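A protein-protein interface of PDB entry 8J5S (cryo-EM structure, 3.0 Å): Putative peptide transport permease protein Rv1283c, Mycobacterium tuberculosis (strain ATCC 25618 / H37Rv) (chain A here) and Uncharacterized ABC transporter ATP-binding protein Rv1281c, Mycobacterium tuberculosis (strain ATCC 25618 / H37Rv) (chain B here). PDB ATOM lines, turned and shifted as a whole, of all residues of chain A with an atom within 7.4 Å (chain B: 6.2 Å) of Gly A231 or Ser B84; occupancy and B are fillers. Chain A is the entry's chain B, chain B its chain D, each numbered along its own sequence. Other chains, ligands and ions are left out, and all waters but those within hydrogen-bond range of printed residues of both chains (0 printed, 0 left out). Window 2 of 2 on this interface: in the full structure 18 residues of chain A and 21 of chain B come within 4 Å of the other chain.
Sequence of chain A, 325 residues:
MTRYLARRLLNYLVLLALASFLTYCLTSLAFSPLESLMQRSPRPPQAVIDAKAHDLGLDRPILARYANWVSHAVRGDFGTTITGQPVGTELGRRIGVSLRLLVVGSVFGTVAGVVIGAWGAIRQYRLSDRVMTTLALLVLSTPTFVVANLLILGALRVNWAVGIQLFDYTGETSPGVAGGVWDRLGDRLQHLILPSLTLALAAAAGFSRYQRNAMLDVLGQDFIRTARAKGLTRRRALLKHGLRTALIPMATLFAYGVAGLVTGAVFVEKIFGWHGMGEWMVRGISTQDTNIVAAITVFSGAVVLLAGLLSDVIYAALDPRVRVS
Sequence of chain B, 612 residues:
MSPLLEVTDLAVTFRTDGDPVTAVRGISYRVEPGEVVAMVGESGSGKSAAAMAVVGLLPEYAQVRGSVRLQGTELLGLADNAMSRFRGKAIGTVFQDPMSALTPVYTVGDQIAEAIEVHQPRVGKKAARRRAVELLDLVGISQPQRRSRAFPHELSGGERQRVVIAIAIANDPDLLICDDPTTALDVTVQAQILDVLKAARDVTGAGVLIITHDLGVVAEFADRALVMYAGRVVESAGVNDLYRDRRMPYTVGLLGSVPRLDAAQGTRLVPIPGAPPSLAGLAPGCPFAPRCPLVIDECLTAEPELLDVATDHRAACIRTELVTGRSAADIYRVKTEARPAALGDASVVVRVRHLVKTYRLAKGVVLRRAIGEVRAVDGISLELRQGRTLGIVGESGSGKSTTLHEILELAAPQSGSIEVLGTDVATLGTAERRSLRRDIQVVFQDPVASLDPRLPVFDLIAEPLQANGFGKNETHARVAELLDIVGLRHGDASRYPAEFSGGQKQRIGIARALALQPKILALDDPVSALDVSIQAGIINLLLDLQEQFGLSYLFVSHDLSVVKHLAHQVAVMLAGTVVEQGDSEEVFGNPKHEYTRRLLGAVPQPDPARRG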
ATOM      1  N   ARG A 225      20.053 -15.996 -21.026  1.00  0.00           N
ATOM      2  CA  ARG A 225      19.099 -16.845 -20.325  1.00  0.00           C
ATOM      3  C   ARG A 225      17.670 -16.426 -20.623  1.00  0.00           C
ATOM      4  O   ARG A 225      16.797 -17.272 -20.831  1.00  0.00           O
ATOM      5  CB  ARG A 225      19.375 -16.797 -18.828  1.00  0.00           C
ATOM      6  CG  ARG A 225      18.370 -17.517 -17.991  1.00  0.00           C
ATOM      7  CD  ARG A 225      18.843 -17.599 -16.563  1.00  0.00           C
ATOM      8  NE  ARG A 225      18.206 -16.603 -15.720  1.00  0.00           N
ATOM      9  CZ  ARG A 225      18.863 -15.782 -14.915  1.00  0.00           C
ATOM     10  NH1 ARG A 225      20.178 -15.840 -14.845  1.00  0.00           N
ATOM     11  NH2 ARG A 225      18.204 -14.906 -14.179  1.00  0.00           N
ATOM     12  N   THR A 226      17.413 -15.121 -20.657  1.00  0.00           N
ATOM     13  CA  THR A 226      16.095 -14.630 -21.036  1.00  0.00           C
ATOM     14  C   THR A 226      15.763 -15.005 -22.469  1.00  0.00           C
ATOM     15  O   THR A 226      14.622 -15.350 -22.779  1.00  0.00           O
ATOM     16  CB  THR A 226      16.040 -13.119 -20.870  1.00  0.00           C
ATOM     17  OG1 THR A 226      16.325 -12.782 -19.512  1.00  0.00           O
ATOM     18  CG2 THR A 226      14.676 -12.596 -21.238  1.00  0.00           C
ATOM     19  N   ALA A 227      16.750 -14.931 -23.358  1.00  0.00           N
ATOM     20  CA  ALA A 227      16.530 -15.287 -24.753  1.00  0.00           C
ATOM     21  C   ALA A 227      16.158 -16.752 -24.903  1.00  0.00           C
ATOM     22  O   ALA A 227      15.298 -17.096 -25.712  1.00  0.00           O
ATOM     23  CB  ALA A 227      17.772 -14.966 -25.575  1.00  0.00           C
ATOM     24  N   ARG A 228      16.807 -17.637 -24.155  1.00  0.00           N
ATOM     25  CA  ARG A 228      16.466 -19.048 -24.262  1.00  0.00           C
ATOM     26  C   ARG A 228      15.306 -19.454 -23.373  1.00  0.00           C
ATOM     27  O   ARG A 228      14.867 -20.600 -23.451  1.00  0.00           O
ATOM     28  CB  ARG A 228      17.669 -19.937 -23.960  1.00  0.00           C
ATOM     29  CG  ARG A 228      18.486 -19.550 -22.788  1.00  0.00           C
ATOM     30  CD  ARG A 228      19.860 -20.156 -22.907  1.00  0.00           C
ATOM     31  NE  ARG A 228      19.789 -21.604 -22.980  1.00  0.00           N
ATOM     32  CZ  ARG A 228      20.002 -22.405 -21.948  1.00  0.00           C
ATOM     33  NH1 ARG A 228      20.308 -21.891 -20.774  1.00  0.00           N
ATOM     34  NH2 ARG A 228      19.913 -23.715 -22.089  1.00  0.00           N
ATOM     35  N   ALA A 229      14.802 -18.554 -22.543  1.00  0.00           N
ATOM     36  CA  ALA A 229      13.594 -18.818 -21.779  1.00  0.00           C
ATOM     37  C   ALA A 229      12.322 -18.515 -22.548  1.00  0.00           C
ATOM     38  O   ALA A 229      11.237 -18.674 -21.990  1.00  0.00           O
ATOM     39  CB  ALA A 229      13.602 -18.011 -20.487  1.00  0.00           C
ATOM     40  N   LYS A 230      12.421 -18.072 -23.799  1.00  0.00           N
ATOM     41  CA  LYS A 230      11.254 -17.843 -24.638  1.00  0.00           C
ATOM     42  C   LYS A 230      11.160 -18.838 -25.780  1.00  0.00           C
ATOM     43  O   LYS A 230      10.309 -18.676 -26.656  1.00  0.00           O
ATOM     44  CB  LYS A 230      11.259 -16.415 -25.185  1.00  0.00           C
ATOM     45  CG  LYS A 230      12.514 -16.046 -25.909  1.00  0.00           C
ATOM     46  CD  LYS A 230      12.350 -14.831 -26.781  1.00  0.00           C
ATOM     47  CE  LYS A 230      12.460 -13.582 -25.957  1.00  0.00           C
ATOM     48  NZ  LYS A 230      12.943 -12.432 -26.741  1.00  0.00           N
ATOM     49  N   GLY A 231      12.006 -19.855 -25.795  1.00  0.00           N
ATOM     50  CA  GLY A 231      11.967 -20.883 -26.799  1.00  0.00           C
ATOM     51  C   GLY A 231      13.102 -20.893 -27.799  1.00  0.00           C
ATOM     52  O   GLY A 231      12.948 -21.489 -28.866  1.00  0.00           O
ATOM     53  N   LEU A 232      14.223 -20.254 -27.500  1.00  0.00           N
ATOM     54  CA  LEU A 232      15.377 -20.241 -28.385  1.00  0.00           C
ATOM     55  C   LEU A 232      16.393 -21.246 -27.868  1.00  0.00           C
ATOM     56  O   LEU A 232      16.861 -21.125 -26.737  1.00  0.00           O
ATOM     57  CB  LEU A 232      15.995 -18.847 -28.458  1.00  0.00           C
ATOM     58  CG  LEU A 232      15.470 -17.876 -29.508  1.00  0.00           C
ATOM     59  CD1 LEU A 232      14.107 -17.370 -29.126  1.00  0.00           C
ATOM     60  CD2 LEU A 232      16.422 -16.722 -29.663  1.00  0.00           C
ATOM     61  N   THR A 233      16.735 -22.230 -28.691  1.00  0.00           N
ATOM     62  CA  THR A 233      17.701 -23.233 -28.278  1.00  0.00           C
ATOM     63  C   THR A 233      19.029 -22.574 -27.938  1.00  0.00           C
ATOM     64  O   THR A 233      19.344 -21.479 -28.398  1.00  0.00           O
ATOM     65  CB  THR A 233      17.894 -24.273 -29.369  1.00  0.00           C
ATOM     66  OG1 THR A 233      18.400 -23.636 -30.543  1.00  0.00           O
ATOM     67  CG2 THR A 233      16.576 -24.931 -29.696  1.00  0.00           C
ATOM     68  N   ARG A 234      19.812 -23.252 -27.104  1.00  0.00           N
ATOM     69  CA  ARG A 234      20.979 -22.607 -26.526  1.00  0.00           C
ATOM     70  C   ARG A 234      22.076 -22.328 -27.536  1.00  0.00           C
ATOM     71  O   ARG A 234      23.003 -21.599 -27.201  1.00  0.00           O
ATOM     72  CB  ARG A 234      21.527 -23.438 -25.372  1.00  0.00           C
ATOM     73  CG  ARG A 234      22.626 -24.398 -25.730  1.00  0.00           C
ATOM     74  CD  ARG A 234      23.241 -25.007 -24.477  1.00  0.00           C
ATOM     75  NE  ARG A 234      24.004 -24.028 -23.711  1.00  0.00           N
ATOM     76  CZ  ARG A 234      25.237 -23.637 -24.013  1.00  0.00           C
ATOM     77  NH1 ARG A 234      25.858 -24.143 -25.067  1.00  0.00           N
ATOM     78  NH2 ARG A 234      25.852 -22.741 -23.258  1.00  0.00           N
ATOM     79  N   ARG A 236      21.202 -21.220 -30.902  1.00  0.00           N
ATOM     80  CA  ARG A 236      20.640 -20.060 -31.573  1.00  0.00           C
ATOM     81  C   ARG A 236      20.666 -18.843 -30.670  1.00  0.00           C
ATOM     82  O   ARG A 236      20.895 -17.725 -31.136  1.00  0.00           O
ATOM     83  CB  ARG A 236      19.215 -20.352 -32.023  1.00  0.00           C
ATOM     84  CG  ARG A 236      18.609 -19.229 -32.806  1.00  0.00           C
ATOM     85  CD  ARG A 236      17.194 -19.536 -33.217  1.00  0.00           C
ATOM     86  NE  ARG A 236      16.625 -18.437 -33.990  1.00  0.00           N
ATOM     87  CZ  ARG A 236      16.524 -18.435 -35.313  1.00  0.00           C
ATOM     88  NH1 ARG A 236      16.949 -19.476 -36.016  1.00  0.00           N
ATOM     89  NH2 ARG A 236      15.995 -17.391 -35.934  1.00  0.00           N
ATOM     90  N   ASP B  80      17.169 -29.935 -24.484  1.00  0.00           N
ATOM     91  CA  ASP B  80      17.204 -28.595 -25.078  1.00  0.00           C
ATOM     92  C   ASP B  80      16.786 -28.611 -26.544  1.00  0.00           C
ATOM     93  O   ASP B  80      17.192 -27.759 -27.331  1.00  0.00           O
ATOM     94  CB  ASP B  80      18.579 -27.946 -24.918  1.00  0.00           C
ATOM     95  CG  ASP B  80      18.567 -26.471 -25.231  1.00  0.00           C
ATOM     96  OD1 ASP B  80      17.476 -25.875 -25.242  1.00  0.00           O
ATOM     97  OD2 ASP B  80      19.646 -25.910 -25.482  1.00  0.00           O
ATOM     98  N   ASN B  81      15.989 -29.588 -26.923  1.00  0.00           N
ATOM     99  CA  ASN B  81      15.293 -29.598 -28.197  1.00  0.00           C
ATOM    100  C   ASN B  81      13.801 -29.745 -28.010  1.00  0.00           C
ATOM    101  O   ASN B  81      13.026 -29.133 -28.748  1.00  0.00           O
ATOM    102  CB  ASN B  81      15.810 -30.727 -29.091  1.00  0.00           C
ATOM    103  CG  ASN B  81      17.024 -30.324 -29.897  1.00  0.00           C
ATOM    104  OD1 ASN B  81      17.574 -29.243 -29.714  1.00  0.00           O
ATOM    105  ND2 ASN B  81      17.451 -31.199 -30.795  1.00  0.00           N
ATOM    106  N   ALA B  82      13.380 -30.556 -27.042  1.00  0.00           N
ATOM    107  CA  ALA B  82      12.018 -30.502 -26.541  1.00  0.00           C
ATOM    108  C   ALA B  82      11.895 -29.544 -25.373  1.00  0.00           C
ATOM    109  O   ALA B  82      10.831 -28.949 -25.174  1.00  0.00           O
ATOM    110  CB  ALA B  82      11.542 -31.893 -26.123  1.00  0.00           C
ATOM    111  N   MET B  83      12.973 -29.374 -24.611  1.00  0.00           N
ATOM    112  CA  MET B  83      12.969 -28.393 -23.536  1.00  0.00           C
ATOM    113  C   MET B  83      12.664 -27.007 -24.073  1.00  0.00           C
ATOM    114  O   MET B  83      11.825 -26.289 -23.521  1.00  0.00           O
ATOM    115  CB  MET B  83      14.310 -28.412 -22.810  1.00  0.00           C
ATOM    116  CG  MET B  83      14.224 -28.064 -21.350  1.00  0.00           C
ATOM    117  SD  MET B  83      13.065 -29.109 -20.478  1.00  0.00           S
ATOM    118  CE  MET B  83      11.814 -27.897 -20.088  1.00  0.00           C
ATOM    119  N   SER B  84      13.328 -26.613 -25.153  1.00  0.00           N
ATOM    120  CA  SER B  84      12.990 -25.360 -25.814  1.00  0.00           C
ATOM    121  C   SER B  84      11.892 -25.554 -26.832  1.00  0.00           C
ATOM    122  O   SER B  84      11.967 -25.073 -27.959  1.00  0.00           O
ATOM    123  CB  SER B  84      14.234 -24.771 -26.457  1.00  0.00           C
ATOM    124  OG  SER B  84      15.191 -24.432 -25.471  1.00  0.00           O
ATOM    125  N   ARG B  85      10.860 -26.283 -26.433  1.00  0.00           N
ATOM    126  CA  ARG B  85       9.576 -26.348 -27.106  1.00  0.00           C
ATOM    127  C   ARG B  85       8.517 -26.251 -26.022  1.00  0.00           C
ATOM    128  O   ARG B  85       7.404 -25.770 -26.250  1.00  0.00           O
ATOM    129  CB  ARG B  85       9.452 -27.635 -27.911  1.00  0.00           C
ATOM    130  CG  ARG B  85       8.038 -28.099 -28.120  1.00  0.00           C
ATOM    131  CD  ARG B  85       7.972 -29.249 -29.104  1.00  0.00           C
ATOM    132  NE  ARG B  85       9.053 -30.208 -28.913  1.00  0.00           N
ATOM    133  CZ  ARG B  85       9.961 -30.504 -29.836  1.00  0.00           C
ATOM    134  NH1 ARG B  85      10.909 -31.391 -29.575  1.00  0.00           N
ATOM    135  NH2 ARG B  85       9.927 -29.910 -31.019  1.00  0.00           N
ATOM    136  N   PHE B  86       8.872 -26.729 -24.828  1.00  0.00           N
ATOM    137  CA  PHE B  86       8.066 -26.430 -23.648  1.00  0.00           C
ATOM    138  C   PHE B  86       8.263 -24.989 -23.217  1.00  0.00           C
ATOM    139  O   PHE B  86       7.298 -24.283 -22.919  1.00  0.00           O
ATOM    140  CB  PHE B  86       8.413 -27.366 -22.488  1.00  0.00           C
ATOM    141  CG  PHE B  86       8.051 -28.794 -22.722  1.00  0.00           C
ATOM    142  CD1 PHE B  86       6.818 -29.281 -22.371  1.00  0.00           C
ATOM    143  CD2 PHE B  86       8.959 -29.650 -23.261  1.00  0.00           C
ATOM    144  CE1 PHE B  86       6.504 -30.589 -22.586  1.00  0.00           C
ATOM    145  CE2 PHE B  86       8.654 -30.952 -23.482  1.00  0.00           C
ATOM    146  CZ  PHE B  86       7.429 -31.427 -23.142  1.00  0.00           C
ATOM    147  N   ARG B  87       9.513 -24.538 -23.185  1.00  0.00           N
ATOM    148  CA  ARG B  87       9.829 -23.198 -22.721  1.00  0.00           C
ATOM    149  C   ARG B  87       9.158 -22.155 -23.595  1.00  0.00           C
ATOM    150  O   ARG B  87       9.204 -22.232 -24.822  1.00  0.00           O
ATOM    151  CB  ARG B  87      11.335 -22.987 -22.732  1.00  0.00           C
ATOM    152  CG  ARG B  87      12.042 -23.444 -21.498  1.00  0.00           C
ATOM    153  CD  ARG B  87      13.456 -22.954 -21.500  1.00  0.00           C
ATOM    154  NE  ARG B  87      14.349 -23.863 -20.803  1.00  0.00           N
ATOM    155  CZ  ARG B  87      15.496 -24.304 -21.296  1.00  0.00           C
ATOM    156  NH1 ARG B  87      15.894 -23.923 -22.493  1.00  0.00           N
ATOM    157  NH2 ARG B  87      16.247 -25.126 -20.592  1.00  0.00           N
ATOM    158  N   GLY B  88       8.545 -21.180 -22.966  1.00  0.00           N
ATOM    159  CA  GLY B  88       7.878 -20.112 -23.691  1.00  0.00           C
ATOM    160  C   GLY B  88       6.437 -20.369 -24.021  1.00  0.00           C
ATOM    161  O   GLY B  88       5.593 -19.498 -23.828  1.00  0.00           O
ATOM    162  N   VAL B 118       8.547 -17.159 -32.240  1.00  0.00           N
ATOM    163  CA  VAL B 118       9.213 -18.465 -32.158  1.00  0.00           C
ATOM    164  C   VAL B 118       8.214 -19.622 -32.124  1.00  0.00           C
ATOM    165  O   VAL B 118       8.408 -20.630 -32.802  1.00  0.00           O
ATOM    166  CB  VAL B 118      10.166 -18.532 -30.955  1.00  0.00           C
ATOM    167  CG1 VAL B 118      10.906 -19.839 -30.980  1.00  0.00           C
ATOM    168  CG2 VAL B 118      11.167 -17.443 -31.040  1.00  0.00           C
ATOM    169  N   HIS B 119       7.153 -19.527 -31.333  1.00  0.00           N
ATOM    170  CA  HIS B 119       6.219 -20.629 -31.158  1.00  0.00           C
ATOM    171  C   HIS B 119       4.995 -20.533 -32.048  1.00  0.00           C
ATOM    172  O   HIS B 119       4.161 -21.441 -32.030  1.00  0.00           O
ATOM    173  CB  HIS B 119       5.787 -20.722 -29.696  1.00  0.00           C
ATOM    174  CG  HIS B 119       6.812 -21.356 -28.812  1.00  0.00           C
ATOM    175  ND1 HIS B 119       7.074 -22.706 -28.828  1.00  0.00           N
ATOM    176  CD2 HIS B 119       7.668 -20.818 -27.916  1.00  0.00           C
ATOM    177  CE1 HIS B 119       8.035 -22.974 -27.966  1.00  0.00           C
ATOM    178  NE2 HIS B 119       8.412 -21.846 -27.399  1.00  0.00           N
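The backbone NH (N) of Arg A234 sits close to the side-chain carboxylate (OD2) of Asp B80, 3.1 Å away.
The side-chain carboxylate of Asp B80 is in hydrogen-bond range of the side-chain hydroxyl of Ser B84, 2.7 Å away. NE2 of His B119 lies within hydrogen-bond range of O of Arg B87 (2.7 Å). The guanidinium group of Arg B87 lies within salt-bridge range of the side-chain carboxylate of Asp B80 (3.7 Å). The guanidinium group (NH1) of Arg B87 is in hydrogen-bond range of the side-chain hydroxyl (OG) of Ser B84, at 3.1 Å.
Arg B87 touches Arg A228 (CD to O, 3.4 Å). Ala A229 touches Gly B88 (O to N, 3.8 Å). His B119 touches Lys A230. Gly A231 touches Ser B84. Arg B87 touches Gly A231 (O to CA, 3.7 Å). Gly A231 touches His B119. Leu A232 touches Ser B84. Leu A232 touches Val B118. CG2 of Thr A233 touches O of Asp B80, at 3.7 Å. Thr A233 touches Ser B84 (CA to OG, 3.95 Å).
Gly A231 touches four residues of chain B. Ser B84 touches just these residues of chain A: Gly A231, Leu A232 and Thr A233. Printed residues of chain B within 4 Å of Arg A228: Arg B87. Printed residues of chain A within 4 Å of Gly B88: Ala A229. Asn B81 touches none of the printed residues of chain A.
Of the 11 printed residues of chain B, 6 touch a printed residue of chain A. Printed residues of chain B that touch a printed residue of chain A: Asp B80, Ser B84, Arg B87, Gly B88, Val B118 and His B119. Hydrophobic or aromatic side chains of chain B within 4 Å of the printed part of chain A: Val B118 and His B119. Hydrophobic or aromatic side chains of chain A that line the printed part of chain B: Leu A232. Among the printed residues, 12 pairs touch across the chains.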
